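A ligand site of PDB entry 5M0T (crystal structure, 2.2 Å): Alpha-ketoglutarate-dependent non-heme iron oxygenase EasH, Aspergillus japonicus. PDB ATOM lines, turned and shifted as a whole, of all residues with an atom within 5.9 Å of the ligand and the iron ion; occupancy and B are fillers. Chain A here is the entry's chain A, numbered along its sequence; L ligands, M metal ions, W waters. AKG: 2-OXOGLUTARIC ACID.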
ATOM      1  N   TYR A  70      27.050   5.173  19.318  1.00  0.00           N
ATOM      2  CA  TYR A  70      25.696   5.532  19.816  1.00  0.00           C
ATOM      3  C   TYR A  70      25.647   6.552  20.982  1.00  0.00           C
ATOM      4  O   TYR A  70      24.634   7.244  21.149  1.00  0.00           O
ATOM      5  CB  TYR A  70      24.912   4.245  20.211  1.00  0.00           C
ATOM      6  CG  TYR A  70      24.556   3.422  18.997  1.00  0.00           C
ATOM      7  CD1 TYR A  70      23.635   3.898  18.051  1.00  0.00           C
ATOM      8  CD2 TYR A  70      25.172   2.198  18.751  1.00  0.00           C
ATOM      9  CE1 TYR A  70      23.323   3.165  16.919  1.00  0.00           C
ATOM     10  CE2 TYR A  70      24.867   1.459  17.618  1.00  0.00           C
ATOM     11  CZ  TYR A  70      23.955   1.942  16.689  1.00  0.00           C
ATOM     12  OH  TYR A  70      23.643   1.194  15.576  1.00  0.00           O
ATOM     13  N   LEU A  71      26.728   6.651  21.774  1.00  0.00           N
ATOM     14  CA  LEU A  71      26.758   7.492  23.003  1.00  0.00           C
ATOM     15  C   LEU A  71      27.513   8.848  22.926  1.00  0.00           C
ATOM     16  O   LEU A  71      27.564   9.575  23.923  1.00  0.00           O
ATOM     17  CB  LEU A  71      27.301   6.668  24.196  1.00  0.00           C
ATOM     18  CG  LEU A  71      26.477   5.439  24.612  1.00  0.00           C
ATOM     19  CD1 LEU A  71      27.262   4.575  25.600  1.00  0.00           C
ATOM     20  CD2 LEU A  71      25.131   5.837  25.210  1.00  0.00           C
ATOM     21  N   MET A  74      26.033  12.644  24.385  1.00  0.00           N
ATOM     22  CA  MET A  74      25.204  12.471  25.582  1.00  0.00           C
ATOM     23  C   MET A  74      26.024  12.736  26.827  1.00  0.00           C
ATOM     24  O   MET A  74      27.253  12.546  26.829  1.00  0.00           O
ATOM     25  CB  MET A  74      24.675  11.055  25.659  1.00  0.00           C
ATOM     26  CG  MET A  74      23.619  10.738  24.619  1.00  0.00           C
ATOM     27  SD  MET A  74      23.000   9.057  24.805  1.00  0.00           S
ATOM     28  CE  MET A  74      21.268   9.310  24.403  1.00  0.00           C
ATOM     29  N   LEU A 120      21.270   8.747  31.292  1.00  0.00           N
ATOM     30  CA  LEU A 120      21.556   9.405  30.019  1.00  0.00           C
ATOM     31  C   LEU A 120      20.764  10.715  29.892  1.00  0.00           C
ATOM     32  O   LEU A 120      19.550  10.685  29.698  1.00  0.00           O
ATOM     33  CB  LEU A 120      21.236   8.475  28.833  1.00  0.00           C
ATOM     34  CG  LEU A 120      22.003   7.150  28.697  1.00  0.00           C
ATOM     35  CD1 LEU A 120      21.563   6.418  27.426  1.00  0.00           C
ATOM     36  CD2 LEU A 120      23.521   7.312  28.698  1.00  0.00           C
ATOM     37  N   GLN A 129      19.424   9.538  18.279  1.00  0.00           N
ATOM     38  CA  GLN A 129      20.156   8.348  17.818  1.00  0.00           C
ATOM     39  C   GLN A 129      19.490   7.786  16.572  1.00  0.00           C
ATOM     40  O   GLN A 129      18.277   7.968  16.355  1.00  0.00           O
ATOM     41  CB  GLN A 129      20.141   7.272  18.907  1.00  0.00           C
ATOM     42  CG  GLN A 129      20.967   7.602  20.119  1.00  0.00           C
ATOM     43  CD  GLN A 129      20.892   6.536  21.213  1.00  0.00           C
ATOM     44  OE1 GLN A 129      19.848   5.958  21.481  1.00  0.00           O
ATOM     45  NE2 GLN A 129      22.014   6.281  21.872  1.00  0.00           N
ATOM     46  N   HIS A 132      18.163   1.362  16.487  1.00  0.00           N
ATOM     47  CA  HIS A 132      19.052   0.203  16.602  1.00  0.00           C
ATOM     48  C   HIS A 132      18.400  -0.849  17.519  1.00  0.00           C
ATOM     49  O   HIS A 132      17.468  -0.537  18.269  1.00  0.00           O
ATOM     50  CB  HIS A 132      20.414   0.651  17.176  1.00  0.00           C
ATOM     51  CG  HIS A 132      20.321   1.274  18.548  1.00  0.00           C
ATOM     52  ND1 HIS A 132      20.062   2.613  18.738  1.00  0.00           N
ATOM     53  CD2 HIS A 132      20.416   0.725  19.780  1.00  0.00           C
ATOM     54  CE1 HIS A 132      20.024   2.863  20.039  1.00  0.00           C
ATOM     55  NE2 HIS A 132      20.205   1.737  20.697  1.00  0.00           N
ATOM     56  N   ARG A 133      18.899  -2.078  17.465  1.00  0.00           N
ATOM     57  CA  ARG A 133      18.492  -3.129  18.393  1.00  0.00           C
ATOM     58  C   ARG A 133      19.616  -3.302  19.395  1.00  0.00           C
ATOM     59  O   ARG A 133      20.793  -3.326  19.018  1.00  0.00           O
ATOM     60  CB  ARG A 133      18.256  -4.437  17.640  1.00  0.00           C
ATOM     61  CG  ARG A 133      17.045  -4.373  16.736  1.00  0.00           C
ATOM     62  CD  ARG A 133      16.692  -5.725  16.154  1.00  0.00           C
ATOM     63  NE  ARG A 133      15.445  -5.640  15.409  1.00  0.00           N
ATOM     64  CZ  ARG A 133      15.330  -5.246  14.135  1.00  0.00           C
ATOM     65  NH1 ARG A 133      16.411  -4.871  13.420  1.00  0.00           N
ATOM     66  NH2 ARG A 133      14.131  -5.214  13.572  1.00  0.00           N
ATOM     67  N   GLU A 134      19.247  -3.426  20.669  1.00  0.00           N
ATOM     68  CA  GLU A 134      20.239  -3.452  21.729  1.00  0.00           C
ATOM     69  C   GLU A 134      21.092  -4.742  21.676  1.00  0.00           C
ATOM     70  O   GLU A 134      22.259  -4.691  22.072  1.00  0.00           O
ATOM     71  CB  GLU A 134      19.587  -3.274  23.110  1.00  0.00           C
ATOM     72  CG  GLU A 134      20.380  -2.321  24.033  1.00  0.00           C
ATOM     73  CD  GLU A 134      20.112  -0.826  23.788  1.00  0.00           C
ATOM     74  OE1 GLU A 134      20.595  -0.253  22.788  1.00  0.00           O
ATOM     75  OE2 GLU A 134      19.392  -0.203  24.611  1.00  0.00           O
ATOM     76  N   ASN A 154      15.646  -4.166  28.487  1.00  0.00           N
ATOM     77  CA  ASN A 154      15.923  -2.788  28.902  1.00  0.00           C
ATOM     78  C   ASN A 154      14.747  -2.152  29.630  1.00  0.00           C
ATOM     79  O   ASN A 154      13.710  -1.918  29.031  1.00  0.00           O
ATOM     80  CB  ASN A 154      16.284  -1.922  27.690  1.00  0.00           C
ATOM     81  CG  ASN A 154      16.927  -0.592  28.081  1.00  0.00           C
ATOM     82  OD1 ASN A 154      16.660  -0.027  29.158  1.00  0.00           O
ATOM     83  ND2 ASN A 154      17.788  -0.082  27.206  1.00  0.00           N
ATOM     84  N   LEU A 156      13.847   1.176  30.754  1.00  0.00           N
ATOM     85  CA  LEU A 156      14.306   2.548  30.564  1.00  0.00           C
ATOM     86  C   LEU A 156      13.367   3.513  31.269  1.00  0.00           C
ATOM     87  O   LEU A 156      12.287   3.824  30.759  1.00  0.00           O
ATOM     88  CB  LEU A 156      14.467   2.880  29.078  1.00  0.00           C
ATOM     89  CG  LEU A 156      15.374   4.096  28.781  1.00  0.00           C
ATOM     90  CD1 LEU A 156      15.863   4.114  27.340  1.00  0.00           C
ATOM     91  CD2 LEU A 156      14.688   5.427  29.104  1.00  0.00           C
ATOM     92  N   PHE A 162       9.158  12.983  29.817  1.00  0.00           N
ATOM     93  CA  PHE A 162       9.557  12.467  28.521  1.00  0.00           C
ATOM     94  C   PHE A 162       8.462  12.902  27.556  1.00  0.00           C
ATOM     95  O   PHE A 162       7.319  12.450  27.687  1.00  0.00           O
ATOM     96  CB  PHE A 162       9.612  10.926  28.549  1.00  0.00           C
ATOM     97  CG  PHE A 162      10.991  10.331  28.626  1.00  0.00           C
ATOM     98  CD1 PHE A 162      11.975  10.892  29.435  1.00  0.00           C
ATOM     99  CD2 PHE A 162      11.289   9.189  27.918  1.00  0.00           C
ATOM    100  CE1 PHE A 162      13.240  10.327  29.501  1.00  0.00           C
ATOM    101  CE2 PHE A 162      12.543   8.611  27.995  1.00  0.00           C
ATOM    102  CZ  PHE A 162      13.534   9.183  28.771  1.00  0.00           C
ATOM    103  N   GLY A 167      12.793  14.705  23.396  1.00  0.00           N
ATOM    104  CA  GLY A 167      13.668  13.574  23.062  1.00  0.00           C
ATOM    105  C   GLY A 167      13.264  12.221  23.633  1.00  0.00           C
ATOM    106  O   GLY A 167      14.101  11.298  23.681  1.00  0.00           O
ATOM    107  N   ALA A 168      12.001  12.063  24.017  1.00  0.00           N
ATOM    108  CA  ALA A 168      11.515  10.765  24.498  1.00  0.00           C
ATOM    109  C   ALA A 168      11.921   9.639  23.548  1.00  0.00           C
ATOM    110  O   ALA A 168      11.837   9.777  22.337  1.00  0.00           O
ATOM    111  CB  ALA A 168       9.992  10.764  24.673  1.00  0.00           C
ATOM    112  N   THR A 169      12.380   8.535  24.151  1.00  0.00           N
ATOM    113  CA  THR A 169      12.880   7.365  23.453  1.00  0.00           C
ATOM    114  C   THR A 169      11.855   6.907  22.435  1.00  0.00           C
ATOM    115  O   THR A 169      10.683   6.816  22.751  1.00  0.00           O
ATOM    116  CB  THR A 169      13.148   6.221  24.451  1.00  0.00           C
ATOM    117  OG1 THR A 169      13.958   6.718  25.510  1.00  0.00           O
ATOM    118  CG2 THR A 169      13.864   5.062  23.799  1.00  0.00           C
ATOM    119  N   PHE A 204      11.662  -2.699  26.773  1.00  0.00           N
ATOM    120  CA  PHE A 204      11.834  -3.351  25.481  1.00  0.00           C
ATOM    121  C   PHE A 204      12.941  -4.414  25.491  1.00  0.00           C
ATOM    122  O   PHE A 204      13.890  -4.315  26.259  1.00  0.00           O
ATOM    123  CB  PHE A 204      12.044  -2.346  24.352  1.00  0.00           C
ATOM    124  CG  PHE A 204      13.148  -1.352  24.600  1.00  0.00           C
ATOM    125  CD1 PHE A 204      14.451  -1.629  24.206  1.00  0.00           C
ATOM    126  CD2 PHE A 204      12.884  -0.126  25.203  1.00  0.00           C
ATOM    127  CE1 PHE A 204      15.475  -0.709  24.422  1.00  0.00           C
ATOM    128  CE2 PHE A 204      13.912   0.798  25.427  1.00  0.00           C
ATOM    129  CZ  PHE A 204      15.198   0.518  25.031  1.00  0.00           C
ATOM    130  N   HIS A 210      14.799   0.831  18.503  1.00  0.00           N
ATOM    131  CA  HIS A 210      14.568   1.983  19.354  1.00  0.00           C
ATOM    132  C   HIS A 210      15.740   2.968  19.211  1.00  0.00           C
ATOM    133  O   HIS A 210      16.786   2.621  18.672  1.00  0.00           O
ATOM    134  CB  HIS A 210      14.493   1.527  20.812  1.00  0.00           C
ATOM    135  CG  HIS A 210      15.810   1.095  21.355  1.00  0.00           C
ATOM    136  ND1 HIS A 210      16.315  -0.171  21.167  1.00  0.00           N
ATOM    137  CD2 HIS A 210      16.778   1.798  21.985  1.00  0.00           C
ATOM    138  CE1 HIS A 210      17.516  -0.240  21.696  1.00  0.00           C
ATOM    139  NE2 HIS A 210      17.832   0.946  22.176  1.00  0.00           N
ATOM    140  N   GLY A 211      15.557   4.182  19.724  1.00  0.00           N
ATOM    141  CA  GLY A 211      16.654   5.139  19.858  1.00  0.00           C
ATOM    142  C   GLY A 211      16.211   6.405  20.554  1.00  0.00           C
ATOM    143  O   GLY A 211      15.037   6.764  20.519  1.00  0.00           O
ATOM    144  N   ALA A 212      17.150   7.077  21.227  1.00  0.00           N
ATOM    145  CA  ALA A 212      16.896   8.347  21.902  1.00  0.00           C
ATOM    146  C   ALA A 212      16.435   9.349  20.866  1.00  0.00           C
ATOM    147  O   ALA A 212      16.993   9.388  19.772  1.00  0.00           O
ATOM    148  CB  ALA A 212      18.131   8.854  22.620  1.00  0.00           C
ATOM    149  N   GLY A 213      15.437  10.150  21.210  1.00  0.00           N
ATOM    150  CA  GLY A 213      14.838  11.104  20.286  1.00  0.00           C
ATOM    151  C   GLY A 213      15.631  12.398  20.215  1.00  0.00           C
ATOM    152  O   GLY A 213      16.541  12.624  21.008  1.00  0.00           O
ATOM    153  N   ARG A 222      16.615  16.376  29.324  1.00  0.00           N
ATOM    154  CA  ARG A 222      15.773  15.162  29.361  1.00  0.00           C
ATOM    155  C   ARG A 222      16.618  14.006  29.919  1.00  0.00           C
ATOM    156  O   ARG A 222      17.581  13.600  29.292  1.00  0.00           O
ATOM    157  CB  ARG A 222      15.216  14.889  27.948  1.00  0.00           C
ATOM    158  CG  ARG A 222      14.558  13.547  27.669  1.00  0.00           C
ATOM    159  CD  ARG A 222      15.602  12.451  27.532  1.00  0.00           C
ATOM    160  NE  ARG A 222      15.280  11.427  26.575  1.00  0.00           N
ATOM    161  CZ  ARG A 222      16.046  10.361  26.359  1.00  0.00           C
ATOM    162  NH1 ARG A 222      17.191  10.143  27.025  1.00  0.00           N
ATOM    163  NH2 ARG A 222      15.652   9.473  25.454  1.00  0.00           N
ATOM    164  N   GLY A 224      17.025  10.186  31.106  1.00  0.00           N
ATOM    165  CA  GLY A 224      16.548   8.802  31.077  1.00  0.00           C
ATOM    166  C   GLY A 224      17.447   7.885  31.878  1.00  0.00           C
ATOM    167  O   GLY A 224      18.580   8.258  32.208  1.00  0.00           O
ATOM    168  N   PRO A 226      18.352   3.969  31.449  1.00  0.00           N
ATOM    169  CA  PRO A 226      18.369   2.605  30.950  1.00  0.00           C
ATOM    170  C   PRO A 226      18.972   1.646  31.960  1.00  0.00           C
ATOM    171  O   PRO A 226      20.017   1.914  32.510  1.00  0.00           O
ATOM    172  CB  PRO A 226      19.269   2.683  29.707  1.00  0.00           C
ATOM    173  CG  PRO A 226      20.078   3.926  29.910  1.00  0.00           C
ATOM    174  CD  PRO A 226      19.101   4.862  30.549  1.00  0.00           C
ATOM    175  N   ILE A 228      19.727  -2.402  31.836  1.00  0.00           N
ATOM    176  CA  ILE A 228      19.662  -3.526  30.903  1.00  0.00           C
ATOM    177  C   ILE A 228      20.080  -4.818  31.601  1.00  0.00           C
ATOM    178  O   ILE A 228      21.216  -4.958  32.064  1.00  0.00           O
ATOM    179  CB  ILE A 228      20.498  -3.271  29.640  1.00  0.00           C
ATOM    180  CG1 ILE A 228      20.248  -1.846  29.120  1.00  0.00           C
ATOM    181  CG2 ILE A 228      20.175  -4.300  28.575  1.00  0.00           C
ATOM    182  CD1 ILE A 228      21.039  -1.469  27.889  1.00  0.00           C
HETATM  183  C1  AKG L   1      21.098   3.160  23.828  1.00  0.00           C
HETATM  184  O1  AKG L   1      21.325   1.998  23.514  1.00  0.00           O
HETATM  185  O2  AKG L   1      22.025   4.033  24.145  1.00  0.00           O
HETATM  186  C2  AKG L   1      19.680   3.743  23.926  1.00  0.00           C
HETATM  187  O5  AKG L   1      18.795   3.192  23.292  1.00  0.00           O
HETATM  188  C3  AKG L   1      19.378   4.922  24.805  1.00  0.00           C
HETATM  189  C4  AKG L   1      17.961   5.432  24.640  1.00  0.00           C
HETATM  190  C5  AKG L   1      17.628   6.640  25.486  1.00  0.00           C
HETATM  191  O3  AKG L   1      18.506   6.977  26.395  1.00  0.00           O
HETATM  192  O4  AKG L   1      16.602   7.250  25.315  1.00  0.00           O
HETATM  193 FE    FE M   1      19.613   1.486  22.523  1.00  0.00          FE
HETATM  194  O   HOH W   1      19.607   1.801  26.243  1.00  0.00           O
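O4 of the ligand lies within salt-bridge range of NH2 of Arg 222.
An oxygen (O4) of the ligand sits at hydrogen-bond distance from the side-chain hydroxyl (OG1) of Thr 169, at 2.7 Å.
The side-chain amide nitrogen (NE2) of Gln 129 is in hydrogen-bond range of an oxygen (O2) of the ligand (3.2 Å).
ND2 of Asn 154 sits at hydrogen-bond distance from OE2 of Glu 134 (3.1 Å).
NH2 of Arg 222 lies within hydrogen-bond range of OG1 of Thr 169 (3.2 Å).
The backbone carbonyl oxygen of Gly 167 lies within hydrogen-bond range of the guanidinium group of Arg 222 (3.0 Å).
N of Gln 129 sits at hydrogen-bond distance from O of Ala 212 (2.9 Å).
The side-chain amide nitrogen (NE2) of Gln 129 sits at hydrogen-bond distance from the backbone carbonyl oxygen (O) of Tyr 70.
The backbone NH (N) of Leu 120 is in hydrogen-bond range of the backbone carbonyl oxygen (O) of Gly 224 (2.9 Å).
The side-chain amide oxygen of Asn 154 lies within hydrogen-bond range of the backbone NH of Leu 156, at 3.5 Å.
Merely in contact with the ligand: Leu 120 (3.3 Å), Ala 212 (3.5 Å), Leu 156 (3.6 Å) and Leu 71 (3.7 Å).
Hydrophobic or aromatic side chains within 4 Å of the ligand: Leu 71, Leu 120, His 132, Leu 156, His 210 and Ala 212.
Of the 23 residues printed, 3 come within 4 Å of the iron ion.
Along chain A the residues within 4 Å of the iron ion span positions 132 to 210.
The iron ion is bound by NE2 of His 210, NE2 of His 132, OE1 of Glu 134, O5 of the ligand and O1 of the ligand.
The iron ion has five donor atoms within binding distance.
Slightly farther from the iron ion lies the side-chain carboxylate (OE2) of Glu 134 (2.7 Å).
Water W1 lies within hydrogen-bond range of the side-chain carboxylate of Glu 134 (2.6 Å) and the side-chain amide nitrogen of Asn 154 (2.8 Å).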
